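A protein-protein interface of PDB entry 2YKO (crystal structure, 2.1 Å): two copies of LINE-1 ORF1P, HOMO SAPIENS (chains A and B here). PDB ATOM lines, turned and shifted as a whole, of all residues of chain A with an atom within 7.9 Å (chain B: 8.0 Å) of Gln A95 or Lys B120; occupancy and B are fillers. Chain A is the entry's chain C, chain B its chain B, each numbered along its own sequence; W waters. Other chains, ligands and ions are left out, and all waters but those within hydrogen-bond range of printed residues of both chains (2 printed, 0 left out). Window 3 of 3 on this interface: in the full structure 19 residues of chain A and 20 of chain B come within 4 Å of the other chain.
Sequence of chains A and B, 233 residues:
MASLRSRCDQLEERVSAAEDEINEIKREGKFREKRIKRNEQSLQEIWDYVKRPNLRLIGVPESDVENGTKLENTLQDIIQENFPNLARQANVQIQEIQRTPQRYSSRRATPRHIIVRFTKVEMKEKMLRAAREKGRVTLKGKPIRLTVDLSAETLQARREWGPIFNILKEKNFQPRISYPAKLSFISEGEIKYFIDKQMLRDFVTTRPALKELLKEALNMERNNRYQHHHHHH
Water W2 bridges NE2 of Gln B93 (2.9 Å) and O of Gln A95 (3.2 Å).
Water W1 lies within hydrogen-bond range of the side-chain carboxylate (OE2) of Glu A96 (3.1 Å) and the side-chain carboxylate (OE1) of Glu B122 (3.4 Å).
Of the 17 printed residues of chain B, 5 touch a printed residue of chain A.
Among the printed residues, 7 pairs touch across the chains.
The backbone carbonyl oxygen (O) of Thr B119 lies within hydrogen-bond range of the side-chain amide nitrogen (NE2) of Gln A95, 3.0 Å away.
The side-chain carboxylate (OE1) of Glu A96 sits at hydrogen-bond distance from the backbone NH (N) of Val B121, at 2.9 Å.
N of Glu B122 sits at hydrogen-bond distance from OE2 of Glu A96 (3.2 Å).
Among the printed residues, merely in contact across the chains: Gly A68 with Glu B122 (3.8 Å), Gln A95 with Gln B95 (3.6 Å), Gln A95 with Lys B120 (3.2 Å) and Glu A96 with Lys B120 (3.4 Å).
The backbone carbonyl oxygen (O) of Gln B93 is in hydrogen-bond range of the backbone NH (N) of Thr B119 (3.1 Å).
The backbone carbonyl oxygen of Arg B117 sits at hydrogen-bond distance from the backbone NH of Gln B95, at 2.8 Å.
O of Phe B118 lies within hydrogen-bond range of NE2 of Gln B95 (2.8 Å).
The side-chain carboxylate (OE2) of Glu B122 is in salt-bridge range of the side-chain amino group (NZ) of Lys B126 (3.9 Å).
The backbone carbonyl oxygen of Arg A117 lies within hydrogen-bond range of the backbone NH of Gln A95 (2.8 Å).
The backbone carbonyl oxygen (O) of Glu A96 sits at hydrogen-bond distance from the backbone NH (N) of Arg A117, at 2.8 Å.
Gln A95 touches just these residues of chain B: Gln B95 (3.6 Å), Thr B119 (3.0 Å) and Lys B120 (3.2 Å).
Of chain A, only Gln A95 (3.2 Å) and Glu A96 (3.4 Å) come within 4 Å of Lys B120.
Of the printed residues of chain A, Val B121 touches Glu A96 (2.9 Å).
Of the printed residues of chain A, Glu B122 touches Gly A68 and Glu A96.
Lys B124 touches none of the printed residues of chain A.
Lys B126 touches none of the printed residues of chain A.
The nearest residue of chain A that does not touch Lys B120 is Glu A72 (4.7 Å).
The nearest printed residue of chain A that does not touch Thr B119 is Glu A96 (4.4 Å).
Gln A95 touches its own counterpart, Gln B95.
Gln A95 touches Thr B119, but with the chains exchanged Thr A119 does not touch Gln B95 (9.0 Å).
Gln A95 touches Lys B120, but with the chains exchanged Lys A120 does not touch Gln B95 (10.9 Å).
10 positions are printed for both chains.
Of the 7 pairs that touch across the chains among the printed residues, 1 has its exchanged pair printed and touching as well.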
ATOM      1  N   PRO A  53      31.581  29.118 -21.248  1.00  0.00           N
ATOM      2  CA  PRO A  53      31.408  28.490 -19.930  1.00  0.00           C
ATOM      3  C   PRO A  53      32.614  27.670 -19.410  1.00  0.00           C
ATOM      4  O   PRO A  53      32.509  27.101 -18.333  1.00  0.00           O
ATOM      5  CB  PRO A  53      30.228  27.552 -20.149  1.00  0.00           C
ATOM      6  CG  PRO A  53      29.668  27.905 -21.526  1.00  0.00           C
ATOM      7  CD  PRO A  53      30.807  28.429 -22.286  1.00  0.00           C
ATOM      8  N   ASN A  54      33.705  27.612 -20.152  1.00  0.00           N
ATOM      9  CA  ASN A  54      34.761  26.625 -19.915  1.00  0.00           C
ATOM     10  C   ASN A  54      35.989  27.267 -19.257  1.00  0.00           C
ATOM     11  O   ASN A  54      36.249  28.452 -19.448  1.00  0.00           O
ATOM     12  CB  ASN A  54      35.237  26.042 -21.258  1.00  0.00           C
ATOM     13  CG  ASN A  54      34.162  25.272 -22.014  1.00  0.00           C
ATOM     14  OD1 ASN A  54      33.053  25.012 -21.522  1.00  0.00           O
ATOM     15  ND2 ASN A  54      34.504  24.888 -23.236  1.00  0.00           N
ATOM     16  N   GLY A  68      34.772  10.959 -15.717  1.00  0.00           N
ATOM     17  CA  GLY A  68      34.262  12.232 -15.239  1.00  0.00           C
ATOM     18  C   GLY A  68      34.303  12.332 -13.727  1.00  0.00           C
ATOM     19  O   GLY A  68      34.648  13.375 -13.185  1.00  0.00           O
ATOM     20  N   THR A  69      33.981  11.244 -13.039  1.00  0.00           N
ATOM     21  CA  THR A  69      33.923  11.285 -11.582  1.00  0.00           C
ATOM     22  C   THR A  69      35.305  11.561 -10.956  1.00  0.00           C
ATOM     23  O   THR A  69      35.433  12.425 -10.069  1.00  0.00           O
ATOM     24  CB  THR A  69      33.267  10.005 -10.997  1.00  0.00           C
ATOM     25  OG1 THR A  69      33.273  10.064  -9.566  1.00  0.00           O
ATOM     26  CG2 THR A  69      34.000   8.779 -11.446  1.00  0.00           C
ATOM     27  N   GLU A  72      36.203  15.246 -11.552  1.00  0.00           N
ATOM     28  CA  GLU A  72      35.404  16.190 -10.790  1.00  0.00           C
ATOM     29  C   GLU A  72      35.880  16.238  -9.310  1.00  0.00           C
ATOM     30  O   GLU A  72      35.929  17.307  -8.704  1.00  0.00           O
ATOM     31  CB  GLU A  72      33.917  15.837 -10.864  1.00  0.00           C
ATOM     32  CG  GLU A  72      33.058  16.836 -10.097  1.00  0.00           C
ATOM     33  CD  GLU A  72      31.568  16.707 -10.358  1.00  0.00           C
ATOM     34  OE1 GLU A  72      31.132  15.630 -10.838  1.00  0.00           O
ATOM     35  OE2 GLU A  72      30.837  17.692 -10.071  1.00  0.00           O
ATOM     36  N   VAL A  92      29.866  24.245  -6.405  1.00  0.00           N
ATOM     37  CA  VAL A  92      30.197  24.609  -7.751  1.00  0.00           C
ATOM     38  C   VAL A  92      29.539  23.614  -8.683  1.00  0.00           C
ATOM     39  O   VAL A  92      29.788  22.408  -8.583  1.00  0.00           O
ATOM     40  CB  VAL A  92      31.690  24.558  -7.905  1.00  0.00           C
ATOM     41  CG1 VAL A  92      32.090  25.048  -9.239  1.00  0.00           C
ATOM     42  CG2 VAL A  92      32.309  25.445  -6.833  1.00  0.00           C
ATOM     43  N   GLN A  93      28.672  24.124  -9.555  1.00  0.00           N
ATOM     44  CA  GLN A  93      27.905  23.316 -10.514  1.00  0.00           C
ATOM     45  C   GLN A  93      28.679  23.099 -11.821  1.00  0.00           C
ATOM     46  O   GLN A  93      28.875  24.042 -12.584  1.00  0.00           O
ATOM     47  CB  GLN A  93      26.599  24.029 -10.862  1.00  0.00           C
ATOM     48  CG  GLN A  93      25.708  24.338  -9.675  1.00  0.00           C
ATOM     49  CD  GLN A  93      25.099  23.098  -9.085  1.00  0.00           C
ATOM     50  OE1 GLN A  93      24.442  22.318  -9.785  1.00  0.00           O
ATOM     51  NE2 GLN A  93      25.318  22.893  -7.791  1.00  0.00           N
ATOM     52  N   ILE A  94      29.113  21.863 -12.056  1.00  0.00           N
ATOM     53  CA  ILE A  94      29.855  21.492 -13.249  1.00  0.00           C
ATOM     54  C   ILE A  94      28.919  20.768 -14.191  1.00  0.00           C
ATOM     55  O   ILE A  94      28.205  19.877 -13.748  1.00  0.00           O
ATOM     56  CB  ILE A  94      31.017  20.544 -12.844  1.00  0.00           C
ATOM     57  CG1 ILE A  94      31.966  21.268 -11.884  1.00  0.00           C
ATOM     58  CG2 ILE A  94      31.795  20.040 -14.041  1.00  0.00           C
ATOM     59  CD1 ILE A  94      32.415  22.608 -12.416  1.00  0.00           C
ATOM     60  N   GLN A  95      28.899  21.139 -15.470  1.00  0.00           N
ATOM     61  CA  GLN A  95      28.078  20.415 -16.430  1.00  0.00           C
ATOM     62  C   GLN A  95      28.844  19.216 -16.924  1.00  0.00           C
ATOM     63  O   GLN A  95      28.300  18.126 -16.971  1.00  0.00           O
ATOM     64  CB  GLN A  95      27.669  21.284 -17.616  1.00  0.00           C
ATOM     65  CG  GLN A  95      27.360  20.452 -18.862  1.00  0.00           C
ATOM     66  CD  GLN A  95      26.833  21.289 -20.032  1.00  0.00           C
ATOM     67  OE1 GLN A  95      26.387  22.421 -19.849  1.00  0.00           O
ATOM     68  NE2 GLN A  95      26.892  20.732 -21.235  1.00  0.00           N
ATOM     69  N   GLU A  96      30.092  19.418 -17.328  1.00  0.00           N
ATOM     70  CA  GLU A  96      30.994  18.287 -17.562  1.00  0.00           C
ATOM     71  C   GLU A  96      32.483  18.641 -17.482  1.00  0.00           C
ATOM     72  O   GLU A  96      32.867  19.804 -17.576  1.00  0.00           O
ATOM     73  CB  GLU A  96      30.717  17.639 -18.906  1.00  0.00           C
ATOM     74  CG  GLU A  96      31.175  16.176 -18.918  1.00  0.00           C
ATOM     75  CD  GLU A  96      30.666  15.432 -20.114  1.00  0.00           C
ATOM     76  OE1 GLU A  96      30.325  16.123 -21.107  1.00  0.00           O
ATOM     77  OE2 GLU A  96      30.581  14.169 -20.054  1.00  0.00           O
ATOM     78  N   ILE A  97      33.326  17.631 -17.297  1.00  0.00           N
ATOM     79  CA  ILE A  97      34.744  17.873 -17.274  1.00  0.00           C
ATOM     80  C   ILE A  97      35.504  16.750 -17.937  1.00  0.00           C
ATOM     81  O   ILE A  97      35.254  15.577 -17.662  1.00  0.00           O
ATOM     82  CB  ILE A  97      35.208  18.055 -15.818  1.00  0.00           C
ATOM     83  CG1 ILE A  97      36.711  18.299 -15.769  1.00  0.00           C
ATOM     84  CG2 ILE A  97      34.869  16.835 -15.004  1.00  0.00           C
ATOM     85  CD1 ILE A  97      37.257  18.623 -14.303  1.00  0.00           C
ATOM     86  N   GLN A  98      36.437  17.085 -18.809  1.00  0.00           N
ATOM     87  CA  GLN A  98      37.172  16.041 -19.522  1.00  0.00           C
ATOM     88  C   GLN A  98      38.505  16.499 -20.087  1.00  0.00           C
ATOM     89  O   GLN A  98      38.742  17.690 -20.275  1.00  0.00           O
ATOM     90  CB  GLN A  98      36.306  15.473 -20.652  1.00  0.00           C
ATOM     91  CG  GLN A  98      35.553  16.492 -21.465  1.00  0.00           C
ATOM     92  CD  GLN A  98      34.417  15.872 -22.304  1.00  0.00           C
ATOM     93  OE1 GLN A  98      34.317  14.643 -22.453  1.00  0.00           O
ATOM     94  NE2 GLN A  98      33.551  16.735 -22.852  1.00  0.00           N
ATOM     95  N   VAL A 116      37.022  22.219 -18.160  1.00  0.00           N
ATOM     96  CA  VAL A 116      35.925  22.197 -17.206  1.00  0.00           C
ATOM     97  C   VAL A 116      34.790  23.059 -17.728  1.00  0.00           C
ATOM     98  O   VAL A 116      34.974  24.256 -17.877  1.00  0.00           O
ATOM     99  CB  VAL A 116      36.323  22.829 -15.876  1.00  0.00           C
ATOM    100  CG1 VAL A 116      35.136  22.744 -14.927  1.00  0.00           C
ATOM    101  CG2 VAL A 116      37.569  22.162 -15.310  1.00  0.00           C
ATOM    102  N   ARG A 117      33.603  22.480 -17.941  1.00  0.00           N
ATOM    103  CA  ARG A 117      32.453  23.275 -18.419  1.00  0.00           C
ATOM    104  C   ARG A 117      31.481  23.511 -17.287  1.00  0.00           C
ATOM    105  O   ARG A 117      30.882  22.571 -16.751  1.00  0.00           O
ATOM    106  CB  ARG A 117      31.737  22.578 -19.586  1.00  0.00           C
ATOM    107  CG  ARG A 117      30.492  23.374 -20.101  1.00  0.00           C
ATOM    108  CD  ARG A 117      30.014  22.912 -21.478  1.00  0.00           C
ATOM    109  NE  ARG A 117      28.927  23.731 -22.034  1.00  0.00           N
ATOM    110  CZ  ARG A 117      28.400  23.553 -23.246  1.00  0.00           C
ATOM    111  NH1 ARG A 117      28.854  22.570 -24.026  1.00  0.00           N
ATOM    112  NH2 ARG A 117      27.419  24.346 -23.687  1.00  0.00           N
ATOM    113  N   PHE A 118      31.370  24.758 -16.883  1.00  0.00           N
ATOM    114  CA  PHE A 118      30.485  25.170 -15.811  1.00  0.00           C
ATOM    115  C   PHE A 118      29.048  25.300 -16.240  1.00  0.00           C
ATOM    116  O   PHE A 118      28.764  25.691 -17.380  1.00  0.00           O
ATOM    117  CB  PHE A 118      30.970  26.521 -15.262  1.00  0.00           C
ATOM    118  CG  PHE A 118      32.212  26.399 -14.453  1.00  0.00           C
ATOM    119  CD1 PHE A 118      32.147  26.108 -13.082  1.00  0.00           C
ATOM    120  CD2 PHE A 118      33.455  26.513 -15.056  1.00  0.00           C
ATOM    121  CE1 PHE A 118      33.311  25.973 -12.338  1.00  0.00           C
ATOM    122  CE2 PHE A 118      34.604  26.351 -14.326  1.00  0.00           C
ATOM    123  CZ  PHE A 118      34.544  26.081 -12.958  1.00  0.00           C
ATOM    124  N   THR A 119      28.131  25.047 -15.317  1.00  0.00           N
ATOM    125  CA  THR A 119      26.711  25.265 -15.614  1.00  0.00           C
ATOM    126  C   THR A 119      26.446  26.761 -15.849  1.00  0.00           C
ATOM    127  O   THR A 119      25.695  27.143 -16.756  1.00  0.00           O
ATOM    128  CB  THR A 119      25.778  24.687 -14.475  1.00  0.00           C
ATOM    129  OG1 THR A 119      26.098  23.302 -14.273  1.00  0.00           O
ATOM    130  CG2 THR A 119      24.343  24.772 -14.908  1.00  0.00           C
ATOM    131  N   LYS A 120      27.035  27.610 -15.013  1.00  0.00           N
ATOM    132  CA  LYS A 120      26.865  29.064 -15.146  1.00  0.00           C
ATOM    133  C   LYS A 120      28.193  29.773 -15.468  1.00  0.00           C
ATOM    134  O   LYS A 120      29.234  29.531 -14.823  1.00  0.00           O
ATOM    135  CB  LYS A 120      26.254  29.614 -13.871  1.00  0.00           C
ATOM    136  CG  LYS A 120      24.987  28.871 -13.502  1.00  0.00           C
ATOM    137  CD  LYS A 120      24.217  29.565 -12.433  1.00  0.00           C
ATOM    138  CE  LYS A 120      23.541  30.811 -12.968  1.00  0.00           C
ATOM    139  NZ  LYS A 120      23.043  31.610 -11.834  1.00  0.00           N
ATOM    140  N   ARG B  52      28.650  16.912 -30.167  1.00  0.00           N
ATOM    141  CA  ARG B  52      29.275  15.775 -29.482  1.00  0.00           C
ATOM    142  C   ARG B  52      28.381  15.055 -28.432  1.00  0.00           C
ATOM    143  O   ARG B  52      28.437  13.860 -28.308  1.00  0.00           O
ATOM    144  CB  ARG B  52      30.559  16.220 -28.792  1.00  0.00           C
ATOM    145  CG  ARG B  52      31.315  15.007 -28.332  1.00  0.00           C
ATOM    146  CD  ARG B  52      32.588  15.326 -27.612  1.00  0.00           C
ATOM    147  NE  ARG B  52      33.257  14.065 -27.284  1.00  0.00           N
ATOM    148  CZ  ARG B  52      34.469  13.982 -26.756  1.00  0.00           C
ATOM    149  NH1 ARG B  52      35.122  15.107 -26.491  1.00  0.00           N
ATOM    150  NH2 ARG B  52      35.013  12.786 -26.483  1.00  0.00           N
ATOM    151  N   PRO B  53      27.549  15.803 -27.687  1.00  0.00           N
ATOM    152  CA  PRO B  53      26.629  15.112 -26.770  1.00  0.00           C
ATOM    153  C   PRO B  53      25.317  14.674 -27.438  1.00  0.00           C
ATOM    154  O   PRO B  53      24.374  14.391 -26.712  1.00  0.00           O
ATOM    155  CB  PRO B  53      26.326  16.158 -25.703  1.00  0.00           C
ATOM    156  CG  PRO B  53      26.444  17.507 -26.429  1.00  0.00           C
ATOM    157  CD  PRO B  53      27.457  17.273 -27.587  1.00  0.00           C
ATOM    158  N   ASN B  54      25.264  14.579 -28.765  1.00  0.00           N
ATOM    159  CA  ASN B  54      23.996  14.305 -29.432  1.00  0.00           C
ATOM    160  C   ASN B  54      23.884  12.834 -29.764  1.00  0.00           C
ATOM    161  O   ASN B  54      24.869  12.153 -30.079  1.00  0.00           O
ATOM    162  CB  ASN B  54      23.769  15.158 -30.720  1.00  0.00           C
ATOM    163  CG  ASN B  54      23.575  16.653 -30.417  1.00  0.00           C
ATOM    164  OD1 ASN B  54      23.847  17.102 -29.304  1.00  0.00           O
ATOM    165  ND2 ASN B  54      23.156  17.429 -31.419  1.00  0.00           N
ATOM    166  N   VAL B  92      19.248  11.162 -16.084  1.00  0.00           N
ATOM    167  CA  VAL B  92      19.336  11.384 -17.530  1.00  0.00           C
ATOM    168  C   VAL B  92      19.043  12.853 -17.867  1.00  0.00           C
ATOM    169  O   VAL B  92      17.896  13.220 -18.153  1.00  0.00           O
ATOM    170  CB  VAL B  92      18.345  10.472 -18.295  1.00  0.00           C
ATOM    171  CG1 VAL B  92      18.380  10.761 -19.794  1.00  0.00           C
ATOM    172  CG2 VAL B  92      18.650   9.001 -18.014  1.00  0.00           C
ATOM    173  N   GLN B  93      20.068  13.699 -17.816  1.00  0.00           N
ATOM    174  CA  GLN B  93      19.842  15.121 -18.030  1.00  0.00           C
ATOM    175  C   GLN B  93      19.919  15.460 -19.523  1.00  0.00           C
ATOM    176  O   GLN B  93      20.792  14.969 -20.223  1.00  0.00           O
ATOM    177  CB  GLN B  93      20.847  15.954 -17.243  1.00  0.00           C
ATOM    178  CG  GLN B  93      21.294  15.348 -15.912  1.00  0.00           C
ATOM    179  CD  GLN B  93      22.394  16.185 -15.250  1.00  0.00           C
ATOM    180  OE1 GLN B  93      22.159  17.335 -14.871  1.00  0.00           O
ATOM    181  NE2 GLN B  93      23.598  15.619 -15.132  1.00  0.00           N
ATOM    182  N   ILE B  94      18.995  16.297 -19.996  1.00  0.00           N
ATOM    183  CA  ILE B  94      18.920  16.693 -21.405  1.00  0.00           C
ATOM    184  C   ILE B  94      18.999  18.235 -21.543  1.00  0.00           C
ATOM    185  O   ILE B  94      18.369  18.983 -20.756  1.00  0.00           O
ATOM    186  CB  ILE B  94      17.577  16.247 -22.053  1.00  0.00           C
ATOM    187  CG1 ILE B  94      17.336  14.738 -21.898  1.00  0.00           C
ATOM    188  CG2 ILE B  94      17.535  16.653 -23.510  1.00  0.00           C
ATOM    189  CD1 ILE B  94      18.455  13.863 -22.392  1.00  0.00           C
ATOM    190  N   GLN B  95      19.774  18.708 -22.515  1.00  0.00           N
ATOM    191  CA  GLN B  95      19.755  20.123 -22.894  1.00  0.00           C
ATOM    192  C   GLN B  95      18.576  20.434 -23.860  1.00  0.00           C
ATOM    193  O   GLN B  95      17.942  21.486 -23.759  1.00  0.00           O
ATOM    194  CB  GLN B  95      21.080  20.564 -23.538  1.00  0.00           C
ATOM    195  CG  GLN B  95      22.368  20.201 -22.783  1.00  0.00           C
ATOM    196  CD  GLN B  95      23.634  20.721 -23.491  1.00  0.00           C
ATOM    197  OE1 GLN B  95      23.747  21.919 -23.762  1.00  0.00           O
ATOM    198  NE2 GLN B  95      24.586  19.816 -23.798  1.00  0.00           N
ATOM    199  N   ARG B 117      19.919  15.891 -27.290  1.00  0.00           N
ATOM    200  CA  ARG B 117      21.136  16.582 -26.903  1.00  0.00           C
ATOM    201  C   ARG B 117      21.311  16.425 -25.405  1.00  0.00           C
ATOM    202  O   ARG B 117      20.639  17.090 -24.627  1.00  0.00           O
ATOM    203  CB  ARG B 117      21.055  18.074 -27.301  1.00  0.00           C
ATOM    204  CG  ARG B 117      22.264  18.900 -26.889  1.00  0.00           C
ATOM    205  CD  ARG B 117      22.211  20.326 -27.421  1.00  0.00           C
ATOM    206  NE  ARG B 117      23.472  21.030 -27.185  1.00  0.00           N
ATOM    207  CZ  ARG B 117      24.604  20.731 -27.810  1.00  0.00           C
ATOM    208  NH1 ARG B 117      24.609  19.751 -28.707  1.00  0.00           N
ATOM    209  NH2 ARG B 117      25.717  21.417 -27.549  1.00  0.00           N
ATOM    210  N   PHE B 118      22.203  15.528 -24.997  1.00  0.00           N
ATOM    211  CA  PHE B 118      22.434  15.294 -23.576  1.00  0.00           C
ATOM    212  C   PHE B 118      23.261  16.375 -22.942  1.00  0.00           C
ATOM    213  O   PHE B 118      24.020  17.071 -23.610  1.00  0.00           O
ATOM    214  CB  PHE B 118      23.123  13.955 -23.341  1.00  0.00           C
ATOM    215  CG  PHE B 118      22.264  12.777 -23.684  1.00  0.00           C
ATOM    216  CD1 PHE B 118      21.306  12.307 -22.790  1.00  0.00           C
ATOM    217  CD2 PHE B 118      22.383  12.172 -24.916  1.00  0.00           C
ATOM    218  CE1 PHE B 118      20.502  11.223 -23.122  1.00  0.00           C
ATOM    219  CE2 PHE B 118      21.605  11.099 -25.243  1.00  0.00           C
ATOM    220  CZ  PHE B 118      20.655  10.626 -24.352  1.00  0.00           C
ATOM    221  N   THR B 119      23.131  16.480 -21.624  1.00  0.00           N
ATOM    222  CA  THR B 119      23.932  17.406 -20.842  1.00  0.00           C
ATOM    223  C   THR B 119      25.385  16.973 -20.769  1.00  0.00           C
ATOM    224  O   THR B 119      26.250  17.819 -20.757  1.00  0.00           O
ATOM    225  CB  THR B 119      23.421  17.517 -19.408  1.00  0.00           C
ATOM    226  OG1 THR B 119      22.141  18.146 -19.411  1.00  0.00           O
ATOM    227  CG2 THR B 119      24.379  18.337 -18.573  1.00  0.00           C
ATOM    228  N   LYS B 120      25.652  15.673 -20.658  1.00  0.00           N
ATOM    229  CA  LYS B 120      27.024  15.179 -20.612  1.00  0.00           C
ATOM    230  C   LYS B 120      27.278  14.234 -21.778  1.00  0.00           C
ATOM    231  O   LYS B 120      26.426  13.409 -22.104  1.00  0.00           O
ATOM    232  CB  LYS B 120      27.296  14.418 -19.317  1.00  0.00           C
ATOM    233  CG  LYS B 120      27.138  15.239 -18.044  1.00  0.00           C
ATOM    234  CD  LYS B 120      27.549  14.426 -16.823  1.00  0.00           C
ATOM    235  CE  LYS B 120      27.691  15.275 -15.570  1.00  0.00           C
ATOM    236  NZ  LYS B 120      28.264  14.474 -14.434  1.00  0.00           N
ATOM    237  N   VAL B 121      28.466  14.330 -22.375  1.00  0.00           N
ATOM    238  CA  VAL B 121      28.847  13.469 -23.479  1.00  0.00           C
ATOM    239  C   VAL B 121      28.796  12.005 -22.990  1.00  0.00           C
ATOM    240  O   VAL B 121      28.390  11.090 -23.716  1.00  0.00           O
ATOM    241  CB  VAL B 121      30.220  13.865 -24.027  1.00  0.00           C
ATOM    242  CG1 VAL B 121      30.713  12.832 -25.023  1.00  0.00           C
ATOM    243  CG2 VAL B 121      30.152  15.316 -24.647  1.00  0.00           C
ATOM    244  N   GLU B 122      29.175  11.810 -21.733  1.00  0.00           N
ATOM    245  CA  GLU B 122      29.131  10.504 -21.076  1.00  0.00           C
ATOM    246  C   GLU B 122      27.771   9.789 -21.189  1.00  0.00           C
ATOM    247  O   GLU B 122      27.709   8.590 -21.433  1.00  0.00           O
ATOM    248  CB  GLU B 122      29.501  10.678 -19.605  1.00  0.00           C
ATOM    249  CG  GLU B 122      30.035   9.424 -18.941  1.00  0.00           C
ATOM    250  CD  GLU B 122      30.258   9.605 -17.439  1.00  0.00           C
ATOM    251  OE1 GLU B 122      31.268  10.241 -17.039  1.00  0.00           O
ATOM    252  OE2 GLU B 122      29.416   9.096 -16.660  1.00  0.00           O
ATOM    253  N   MET B 123      26.674  10.511 -21.035  1.00  0.00           N
ATOM    254  CA  MET B 123      25.350   9.892 -21.184  1.00  0.00           C
ATOM    255  C   MET B 123      25.109   9.412 -22.616  1.00  0.00           C
ATOM    256  O   MET B 123      24.513   8.345 -22.836  1.00  0.00           O
ATOM    257  CB  MET B 123      24.240  10.870 -20.788  1.00  0.00           C
ATOM    258  CG  MET B 123      23.641  10.604 -19.405  1.00  0.00           C
ATOM    259  SD  MET B 123      22.843   8.801 -19.285  1.00  0.00           S
ATOM    260  CE  MET B 123      21.744   8.846 -20.877  1.00  0.00           C
ATOM    261  N   LYS B 124      25.548  10.196 -23.599  1.00  0.00           N
ATOM    262  CA  LYS B 124      25.371   9.779 -24.995  1.00  0.00           C
ATOM    263  C   LYS B 124      26.130   8.458 -25.204  1.00  0.00           C
ATOM    264  O   LYS B 124      25.638   7.500 -25.819  1.00  0.00           O
ATOM    265  CB  LYS B 124      25.934  10.820 -25.970  1.00  0.00           C
ATOM    266  CG  LYS B 124      25.861  10.330 -27.452  1.00  0.00           C
ATOM    267  CD  LYS B 124      26.930  10.930 -28.320  1.00  0.00           C
ATOM    268  CE  LYS B 124      28.298  10.471 -27.859  1.00  0.00           C
ATOM    269  NZ  LYS B 124      29.393  11.204 -28.582  1.00  0.00           N
ATOM    270  N   GLU B 125      27.351   8.427 -24.687  1.00  0.00           N
ATOM    271  CA  GLU B 125      28.185   7.240 -24.830  1.00  0.00           C
ATOM    272  C   GLU B 125      27.514   6.017 -24.207  1.00  0.00           C
ATOM    273  O   GLU B 125      27.532   4.959 -24.796  1.00  0.00           O
ATOM    274  CB  GLU B 125      29.567   7.459 -24.222  1.00  0.00           C
ATOM    275  CG  GLU B 125      30.413   8.448 -25.013  1.00  0.00           C
ATOM    276  CD  GLU B 125      31.597   8.983 -24.195  1.00  0.00           C
ATOM    277  OE1 GLU B 125      31.737   8.565 -23.030  1.00  0.00           O
ATOM    278  OE2 GLU B 125      32.370   9.825 -24.696  1.00  0.00           O
ATOM    279  N   LYS B 126      26.919   6.167 -23.030  1.00  0.00           N
ATOM    280  CA  LYS B 126      26.330   5.017 -22.353  1.00  0.00           C
ATOM    281  C   LYS B 126      25.098   4.523 -23.108  1.00  0.00           C
ATOM    282  O   LYS B 126      24.800   3.338 -23.108  1.00  0.00           O
ATOM    283  CB  LYS B 126      25.965   5.336 -20.895  1.00  0.00           C
ATOM    284  CG  LYS B 126      27.160   5.513 -19.991  1.00  0.00           C
ATOM    285  CD  LYS B 126      26.756   5.761 -18.524  1.00  0.00           C
ATOM    286  CE  LYS B 126      25.979   7.070 -18.356  1.00  0.00           C
ATOM    287  NZ  LYS B 126      25.845   7.448 -16.914  1.00  0.00           N
HETATM  288  O   HOH W   1      31.690  13.582 -17.262  1.00  0.00           O
HETATM  289  O   HOH W   2      25.568  17.770 -15.267  1.00  0.00           O
